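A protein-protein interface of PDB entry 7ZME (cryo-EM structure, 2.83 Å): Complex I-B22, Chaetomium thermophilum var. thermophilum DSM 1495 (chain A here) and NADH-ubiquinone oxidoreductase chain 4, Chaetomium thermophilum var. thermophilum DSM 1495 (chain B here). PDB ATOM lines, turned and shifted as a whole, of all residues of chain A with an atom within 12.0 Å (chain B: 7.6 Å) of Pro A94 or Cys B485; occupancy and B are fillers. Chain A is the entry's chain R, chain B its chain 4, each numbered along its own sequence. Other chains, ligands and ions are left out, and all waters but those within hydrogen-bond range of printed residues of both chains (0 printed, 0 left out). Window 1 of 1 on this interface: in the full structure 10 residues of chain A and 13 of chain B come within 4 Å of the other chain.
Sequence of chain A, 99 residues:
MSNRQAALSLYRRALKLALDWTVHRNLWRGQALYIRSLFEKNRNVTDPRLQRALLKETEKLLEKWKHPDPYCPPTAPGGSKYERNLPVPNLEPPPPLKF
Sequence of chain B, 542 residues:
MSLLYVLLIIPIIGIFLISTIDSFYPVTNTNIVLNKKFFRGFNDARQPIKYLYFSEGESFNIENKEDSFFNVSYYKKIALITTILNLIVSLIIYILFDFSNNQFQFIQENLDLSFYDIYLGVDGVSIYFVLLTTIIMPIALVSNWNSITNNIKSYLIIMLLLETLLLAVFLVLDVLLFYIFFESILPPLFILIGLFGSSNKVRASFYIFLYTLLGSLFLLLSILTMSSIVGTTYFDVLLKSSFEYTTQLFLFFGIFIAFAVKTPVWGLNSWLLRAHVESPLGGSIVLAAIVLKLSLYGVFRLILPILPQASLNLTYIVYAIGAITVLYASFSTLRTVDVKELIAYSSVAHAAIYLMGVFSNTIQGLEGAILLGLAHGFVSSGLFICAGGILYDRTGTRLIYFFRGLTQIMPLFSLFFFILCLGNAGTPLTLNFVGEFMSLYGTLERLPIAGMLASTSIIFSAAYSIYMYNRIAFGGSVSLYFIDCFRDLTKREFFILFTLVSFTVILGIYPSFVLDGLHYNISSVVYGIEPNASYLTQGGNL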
ATOM      1  N   PRO A  87       1.008   1.410 -13.266  1.00  0.00           N
ATOM      2  CA  PRO A  87       2.076   0.414 -13.142  1.00  0.00           C
ATOM      3  C   PRO A  87       3.419   0.982 -13.567  1.00  0.00           C
ATOM      4  O   PRO A  87       3.508   2.002 -14.252  1.00  0.00           O
ATOM      5  CB  PRO A  87       1.625  -0.703 -14.084  1.00  0.00           C
ATOM      6  CG  PRO A  87       0.829   0.008 -15.124  1.00  0.00           C
ATOM      7  CD  PRO A  87       0.141   1.150 -14.428  1.00  0.00           C
ATOM      8  N   VAL A  88       4.477   0.299 -13.143  1.00  0.00           N
ATOM      9  CA  VAL A  88       5.824   0.724 -13.538  1.00  0.00           C
ATOM     10  C   VAL A  88       5.966   0.575 -15.045  1.00  0.00           C
ATOM     11  O   VAL A  88       5.407  -0.373 -15.632  1.00  0.00           O
ATOM     12  CB  VAL A  88       6.895  -0.099 -12.807  1.00  0.00           C
ATOM     13  CG1 VAL A  88       6.797   0.099 -11.297  1.00  0.00           C
ATOM     14  CG2 VAL A  88       6.786  -1.555 -13.190  1.00  0.00           C
ATOM     15  N   PRO A  89       6.666   1.480 -15.728  1.00  0.00           N
ATOM     16  CA  PRO A  89       6.855   1.290 -17.173  1.00  0.00           C
ATOM     17  C   PRO A  89       7.774   0.130 -17.507  1.00  0.00           C
ATOM     18  O   PRO A  89       7.498  -0.621 -18.451  1.00  0.00           O
ATOM     19  CB  PRO A  89       7.439   2.638 -17.623  1.00  0.00           C
ATOM     20  CG  PRO A  89       7.094   3.599 -16.521  1.00  0.00           C
ATOM     21  CD  PRO A  89       7.134   2.796 -15.272  1.00  0.00           C
ATOM     22  N   ASN A  90       8.855  -0.044 -16.755  1.00  0.00           N
ATOM     23  CA  ASN A  90       9.890  -1.029 -17.056  1.00  0.00           C
ATOM     24  C   ASN A  90       9.755  -2.196 -16.088  1.00  0.00           C
ATOM     25  O   ASN A  90      10.130  -2.084 -14.918  1.00  0.00           O
ATOM     26  CB  ASN A  90      11.272  -0.387 -16.950  1.00  0.00           C
ATOM     27  CG  ASN A  90      12.348  -1.194 -17.631  1.00  0.00           C
ATOM     28  OD1 ASN A  90      12.209  -2.397 -17.831  1.00  0.00           O
ATOM     29  ND2 ASN A  90      13.435  -0.531 -17.997  1.00  0.00           N
ATOM     30  N   LEU A  91       9.224  -3.317 -16.573  1.00  0.00           N
ATOM     31  CA  LEU A  91       9.044  -4.482 -15.718  1.00  0.00           C
ATOM     32  C   LEU A  91      10.287  -5.352 -15.627  1.00  0.00           C
ATOM     33  O   LEU A  91      10.342  -6.230 -14.760  1.00  0.00           O
ATOM     34  CB  LEU A  91       7.873  -5.334 -16.211  1.00  0.00           C
ATOM     35  CG  LEU A  91       6.460  -4.925 -15.790  1.00  0.00           C
ATOM     36  CD1 LEU A  91       6.311  -5.030 -14.289  1.00  0.00           C
ATOM     37  CD2 LEU A  91       6.082  -3.537 -16.278  1.00  0.00           C
ATOM     38  N   GLU A  92      11.279  -5.131 -16.488  1.00  0.00           N
ATOM     39  CA  GLU A  92      12.478  -5.948 -16.510  1.00  0.00           C
ATOM     40  C   GLU A  92      13.394  -5.611 -15.337  1.00  0.00           C
ATOM     41  O   GLU A  92      13.451  -4.461 -14.894  1.00  0.00           O
ATOM     42  CB  GLU A  92      13.229  -5.753 -17.820  1.00  0.00           C
ATOM     43  CG  GLU A  92      12.739  -6.636 -18.957  1.00  0.00           C
ATOM     44  CD  GLU A  92      11.449  -6.135 -19.581  1.00  0.00           C
ATOM     45  OE1 GLU A  92      10.934  -5.087 -19.139  1.00  0.00           O
ATOM     46  OE2 GLU A  92      10.952  -6.794 -20.518  1.00  0.00           O
ATOM     47  N   PRO A  93      14.116  -6.600 -14.821  1.00  0.00           N
ATOM     48  CA  PRO A  93      15.035  -6.355 -13.706  1.00  0.00           C
ATOM     49  C   PRO A  93      16.214  -5.505 -14.142  1.00  0.00           C
ATOM     50  O   PRO A  93      16.543  -5.444 -15.335  1.00  0.00           O
ATOM     51  CB  PRO A  93      15.490  -7.766 -13.306  1.00  0.00           C
ATOM     52  CG  PRO A  93      14.480  -8.687 -13.897  1.00  0.00           C
ATOM     53  CD  PRO A  93      14.014  -8.030 -15.151  1.00  0.00           C
ATOM     54  N   PRO A  94      16.865  -4.822 -13.202  1.00  0.00           N
ATOM     55  CA  PRO A  94      18.031  -4.028 -13.557  1.00  0.00           C
ATOM     56  C   PRO A  94      19.143  -4.906 -14.097  1.00  0.00           C
ATOM     57  O   PRO A  94      19.329  -6.052 -13.649  1.00  0.00           O
ATOM     58  CB  PRO A  94      18.432  -3.371 -12.227  1.00  0.00           C
ATOM     59  CG  PRO A  94      17.654  -4.075 -11.176  1.00  0.00           C
ATOM     60  CD  PRO A  94      16.418  -4.555 -11.828  1.00  0.00           C
ATOM     61  N   PRO A  95      19.915  -4.402 -15.052  1.00  0.00           N
ATOM     62  CA  PRO A  95      21.094  -5.125 -15.520  1.00  0.00           C
ATOM     63  C   PRO A  95      22.146  -5.185 -14.431  1.00  0.00           C
ATOM     64  O   PRO A  95      22.171  -4.330 -13.535  1.00  0.00           O
ATOM     65  CB  PRO A  95      21.571  -4.278 -16.707  1.00  0.00           C
ATOM     66  CG  PRO A  95      21.102  -2.910 -16.377  1.00  0.00           C
ATOM     67  CD  PRO A  95      19.778  -3.090 -15.705  1.00  0.00           C
ATOM     68  N   PRO A  96      23.036  -6.169 -14.469  1.00  0.00           N
ATOM     69  CA  PRO A  96      24.007  -6.305 -13.377  1.00  0.00           C
ATOM     70  C   PRO A  96      25.040  -5.193 -13.385  1.00  0.00           C
ATOM     71  O   PRO A  96      25.969  -5.194 -14.196  1.00  0.00           O
ATOM     72  CB  PRO A  96      24.650  -7.671 -13.650  1.00  0.00           C
ATOM     73  CG  PRO A  96      24.466  -7.891 -15.112  1.00  0.00           C
ATOM     74  CD  PRO A  96      23.163  -7.242 -15.469  1.00  0.00           C
ATOM     75  N   LEU A  97      24.885  -4.246 -12.463  1.00  0.00           N
ATOM     76  CA  LEU A  97      25.815  -3.142 -12.277  1.00  0.00           C
ATOM     77  C   LEU A  97      26.159  -3.030 -10.802  1.00  0.00           C
ATOM     78  O   LEU A  97      25.314  -3.284  -9.939  1.00  0.00           O
ATOM     79  CB  LEU A  97      25.234  -1.811 -12.764  1.00  0.00           C
ATOM     80  CG  LEU A  97      25.589  -1.277 -14.152  1.00  0.00           C
ATOM     81  CD1 LEU A  97      25.319  -2.301 -15.239  1.00  0.00           C
ATOM     82  CD2 LEU A  97      24.838   0.008 -14.425  1.00  0.00           C
ATOM     83  N   LYS A  98      27.386  -2.609 -10.504  1.00  0.00           N
ATOM     84  CA  LYS A  98      27.756  -2.406  -9.079  1.00  0.00           C
ATOM     85  C   LYS A  98      27.768  -0.911  -8.755  1.00  0.00           C
ATOM     86  O   LYS A  98      28.388  -0.150  -9.521  1.00  0.00           O
ATOM     87  CB  LYS A  98      29.117  -3.042  -8.777  1.00  0.00           C
ATOM     88  CG  LYS A  98      29.082  -4.505  -8.357  1.00  0.00           C
ATOM     89  CD  LYS A  98      28.787  -5.466  -9.490  1.00  0.00           C
ATOM     90  CE  LYS A  98      28.755  -6.912  -9.045  1.00  0.00           C
ATOM     91  NZ  LYS A  98      28.510  -7.830 -10.182  1.00  0.00           N
ATOM     92  N   PHE A  99      27.064  -0.511  -7.695  1.00  0.00           N
ATOM     93  CA  PHE A  99      27.143   0.902  -7.239  1.00  0.00           C
ATOM     94  C   PHE A  99      27.544   0.888  -5.760  1.00  0.00           C
ATOM     95  O   PHE A  99      28.618   1.439  -5.464  1.00  0.00           O
ATOM     96  CB  PHE A  99      25.815   1.626  -7.469  1.00  0.00           C
ATOM     97  CG  PHE A  99      25.379   1.647  -8.906  1.00  0.00           C
ATOM     98  CD1 PHE A  99      25.954   2.527  -9.804  1.00  0.00           C
ATOM     99  CD2 PHE A  99      24.408   0.776  -9.361  1.00  0.00           C
ATOM    100  CE1 PHE A  99      25.564   2.538 -11.131  1.00  0.00           C
ATOM    101  CE2 PHE A  99      24.023   0.792 -10.689  1.00  0.00           C
ATOM    102  CZ  PHE A  99      24.589   1.682 -11.566  1.00  0.00           C
ATOM    103  N   GLN B 408       8.375   3.915  -6.943  1.00  0.00           N
ATOM    104  CA  GLN B 408       7.883   2.682  -7.541  1.00  0.00           C
ATOM    105  C   GLN B 408       8.976   1.629  -7.640  1.00  0.00           C
ATOM    106  O   GLN B 408       8.688   0.429  -7.595  1.00  0.00           O
ATOM    107  CB  GLN B 408       7.290   2.971  -8.918  1.00  0.00           C
ATOM    108  CG  GLN B 408       5.854   3.443  -8.872  1.00  0.00           C
ATOM    109  CD  GLN B 408       5.121   3.211 -10.169  1.00  0.00           C
ATOM    110  OE1 GLN B 408       5.660   3.439 -11.246  1.00  0.00           O
ATOM    111  NE2 GLN B 408       3.879   2.760 -10.072  1.00  0.00           N
ATOM    112  N   ILE B 409      10.229   2.057  -7.761  1.00  0.00           N
ATOM    113  CA  ILE B 409      11.341   1.143  -7.935  1.00  0.00           C
ATOM    114  C   ILE B 409      12.233   1.062  -6.700  1.00  0.00           C
ATOM    115  O   ILE B 409      12.799  -0.003  -6.433  1.00  0.00           O
ATOM    116  CB  ILE B 409      12.158   1.550  -9.182  1.00  0.00           C
ATOM    117  CG1 ILE B 409      11.318   1.333 -10.430  1.00  0.00           C
ATOM    118  CG2 ILE B 409      13.441   0.752  -9.303  1.00  0.00           C
ATOM    119  CD1 ILE B 409      10.657  -0.023 -10.462  1.00  0.00           C
ATOM    120  N   VAL B 478       7.220   6.415 -13.061  1.00  0.00           N
ATOM    121  CA  VAL B 478       8.677   6.338 -13.092  1.00  0.00           C
ATOM    122  C   VAL B 478       9.119   7.195 -14.263  1.00  0.00           C
ATOM    123  O   VAL B 478       8.447   7.232 -15.298  1.00  0.00           O
ATOM    124  CB  VAL B 478       9.208   4.889 -13.241  1.00  0.00           C
ATOM    125  CG1 VAL B 478      10.689   4.888 -13.570  1.00  0.00           C
ATOM    126  CG2 VAL B 478       8.998   4.069 -11.985  1.00  0.00           C
ATOM    127  N   PHE B 482      14.424   6.816 -17.961  1.00  0.00           N
ATOM    128  CA  PHE B 482      15.095   5.625 -17.448  1.00  0.00           C
ATOM    129  C   PHE B 482      14.712   4.461 -18.345  1.00  0.00           C
ATOM    130  O   PHE B 482      13.714   3.775 -18.119  1.00  0.00           O
ATOM    131  CB  PHE B 482      14.717   5.354 -15.997  1.00  0.00           C
ATOM    132  CG  PHE B 482      15.039   6.476 -15.060  1.00  0.00           C
ATOM    133  CD1 PHE B 482      16.051   7.368 -15.346  1.00  0.00           C
ATOM    134  CD2 PHE B 482      14.326   6.637 -13.890  1.00  0.00           C
ATOM    135  CE1 PHE B 482      16.348   8.397 -14.483  1.00  0.00           C
ATOM    136  CE2 PHE B 482      14.616   7.668 -13.024  1.00  0.00           C
ATOM    137  CZ  PHE B 482      15.631   8.548 -13.317  1.00  0.00           C
ATOM    138  N   ILE B 483      15.521   4.232 -19.382  1.00  0.00           N
ATOM    139  CA  ILE B 483      15.327   3.075 -20.253  1.00  0.00           C
ATOM    140  C   ILE B 483      15.900   1.807 -19.653  1.00  0.00           C
ATOM    141  O   ILE B 483      15.893   0.758 -20.311  1.00  0.00           O
ATOM    142  CB  ILE B 483      15.962   3.320 -21.635  1.00  0.00           C
ATOM    143  CG1 ILE B 483      17.468   3.505 -21.491  1.00  0.00           C
ATOM    144  CG2 ILE B 483      15.335   4.529 -22.302  1.00  0.00           C
ATOM    145  CD1 ILE B 483      18.199   3.531 -22.796  1.00  0.00           C
ATOM    146  N   ASP B 484      16.387   1.869 -18.422  1.00  0.00           N
ATOM    147  CA  ASP B 484      17.081   0.754 -17.801  1.00  0.00           C
ATOM    148  C   ASP B 484      16.728   0.779 -16.323  1.00  0.00           C
ATOM    149  O   ASP B 484      17.141   1.698 -15.611  1.00  0.00           O
ATOM    150  CB  ASP B 484      18.588   0.889 -18.013  1.00  0.00           C
ATOM    151  CG  ASP B 484      19.282  -0.436 -18.120  1.00  0.00           C
ATOM    152  OD1 ASP B 484      18.585  -1.471 -18.091  1.00  0.00           O
ATOM    153  OD2 ASP B 484      20.524  -0.441 -18.255  1.00  0.00           O
ATOM    154  N   CYS B 485      15.964  -0.211 -15.867  1.00  0.00           N
ATOM    155  CA  CYS B 485      15.434  -0.173 -14.511  1.00  0.00           C
ATOM    156  C   CYS B 485      16.571  -0.146 -13.494  1.00  0.00           C
ATOM    157  O   CYS B 485      17.657  -0.683 -13.727  1.00  0.00           O
ATOM    158  CB  CYS B 485      14.518  -1.373 -14.261  1.00  0.00           C
ATOM    159  SG  CYS B 485      13.577  -1.304 -12.716  1.00  0.00           S
ATOM    160  N   PHE B 486      16.324   0.515 -12.370  1.00  0.00           N
ATOM    161  CA  PHE B 486      17.343   0.745 -11.357  1.00  0.00           C
ATOM    162  C   PHE B 486      17.287  -0.330 -10.281  1.00  0.00           C
ATOM    163  O   PHE B 486      16.316  -1.076 -10.154  1.00  0.00           O
ATOM    164  CB  PHE B 486      17.168   2.122 -10.707  1.00  0.00           C
ATOM    165  CG  PHE B 486      17.465   3.276 -11.615  1.00  0.00           C
ATOM    166  CD1 PHE B 486      17.943   3.071 -12.894  1.00  0.00           C
ATOM    167  CD2 PHE B 486      17.254   4.573 -11.184  1.00  0.00           C
ATOM    168  CE1 PHE B 486      18.210   4.129 -13.723  1.00  0.00           C
ATOM    169  CE2 PHE B 486      17.521   5.639 -12.010  1.00  0.00           C
ATOM    170  CZ  PHE B 486      18.001   5.416 -13.281  1.00  0.00           C
ATOM    171  N   ARG B 487      18.352  -0.396  -9.495  1.00  0.00           N
ATOM    172  CA  ARG B 487      18.353  -1.155  -8.258  1.00  0.00           C
ATOM    173  C   ARG B 487      18.137  -0.203  -7.090  1.00  0.00           C
ATOM    174  O   ARG B 487      18.468   0.983  -7.163  1.00  0.00           O
ATOM    175  CB  ARG B 487      19.660  -1.928  -8.077  1.00  0.00           C
ATOM    176  CG  ARG B 487      20.903  -1.065  -8.113  1.00  0.00           C
ATOM    177  CD  ARG B 487      22.155  -1.903  -7.968  1.00  0.00           C
ATOM    178  NE  ARG B 487      22.007  -2.938  -6.954  1.00  0.00           N
ATOM    179  CZ  ARG B 487      22.972  -3.777  -6.598  1.00  0.00           C
ATOM    180  NH1 ARG B 487      22.750  -4.687  -5.664  1.00  0.00           N
ATOM    181  NH2 ARG B 487      24.159  -3.708  -7.176  1.00  0.00           N
ATOM    182  N   ASP B 488      17.578  -0.733  -6.011  1.00  0.00           N
ATOM    183  CA  ASP B 488      17.270   0.063  -4.832  1.00  0.00           C
ATOM    184  C   ASP B 488      18.558   0.291  -4.044  1.00  0.00           C
ATOM    185  O   ASP B 488      19.664   0.054  -4.534  1.00  0.00           O
ATOM    186  CB  ASP B 488      16.181  -0.626  -4.012  1.00  0.00           C
ATOM    187  CG  ASP B 488      15.587   0.270  -2.939  1.00  0.00           C
ATOM    188  OD1 ASP B 488      15.895   1.476  -2.929  1.00  0.00           O
ATOM    189  OD2 ASP B 488      14.826  -0.240  -2.095  1.00  0.00           O
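Printed residues of chain B that touch a printed residue of chain A: Gln B408, Ile B409, Val B478, Ile B483, Asp B484, Cys B485, Phe B486 and Arg B487.
Hydrophobic or aromatic side chains of chain B within 4 Å of the printed part of chain A: Ile B409 and Val B478.
Hydrophobic or aromatic side chains of chain A within 4 Å of the printed part of chain B: Val A88, Pro A89, Pro A94, Pro A95 and Phe A99.
Among the printed residues, no Asp or Glu carboxylate lies within 4 Å of a Lys or Arg side-chain nitrogen of the other chain.
OD1 of Asn A90 lies within hydrogen-bond range of N of Glu A92 (3.2 Å).
Pro A94 touches just these residues of chain B: Cys B485 (3.2 Å) and Phe B486 (3.4 Å).
Cys B485 touches just these residues of chain A: Asn A90, Glu A92, Pro A94 and Pro A95.
Asp B484 touches two residues of chain A.
Of the printed residues of chain A, Phe B486 touches Pro A94.
Of the printed residues of chain A, Arg B487 touches Leu A97 and Phe A99.
Of the printed residues of chain B, Val A88 touches Gln B408 and Ile B409.
Of the printed residues of chain A, Val B478 touches Pro A89.
Printed residues of chain B within 4 Å of Glu A92: Cys B485.
Of the printed residues of chain B, Asn A90 touches Ile B483 (3.6 Å), Asp B484 (3.8 Å) and Cys B485 (3.3 Å).
Phe B482 touches none of the printed residues of chain A.
Pro A93 touches none of the printed residues of chain B.
NE2 of Gln B408 touches C of Pro A87, at 3.9 Å.
OE1 of Gln B408 touches CG1 of Val A88, at 3.5 Å.
Val A88 touches Ile B409 (CG1 to CD1, 3.95 Å).
Pro A89 touches Val B478.
ND2 of Asn A90 touches O of Ile B483, at 3.6 Å.
ND2 of Asn A90 touches N of Asp B484, at 3.8 Å.
Glu A92 touches Cys B485 (O to CB, 3.3 Å).
O of Cys B485 touches CB of Pro A94, 3.2 Å away.
O of Phe B486 touches CG of Pro A94 (3.4 Å).
O of Cys B485 touches CD of Pro A95, 3.8 Å away.
N of Cys B485 sits close to ND2 of Asn A90, 3.3 Å away.
The backbone carbonyl oxygen (O) of Leu A97 lies within hydrogen-bond range of the guanidinium group (NH2) of Arg B487, at 3.0 Å.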
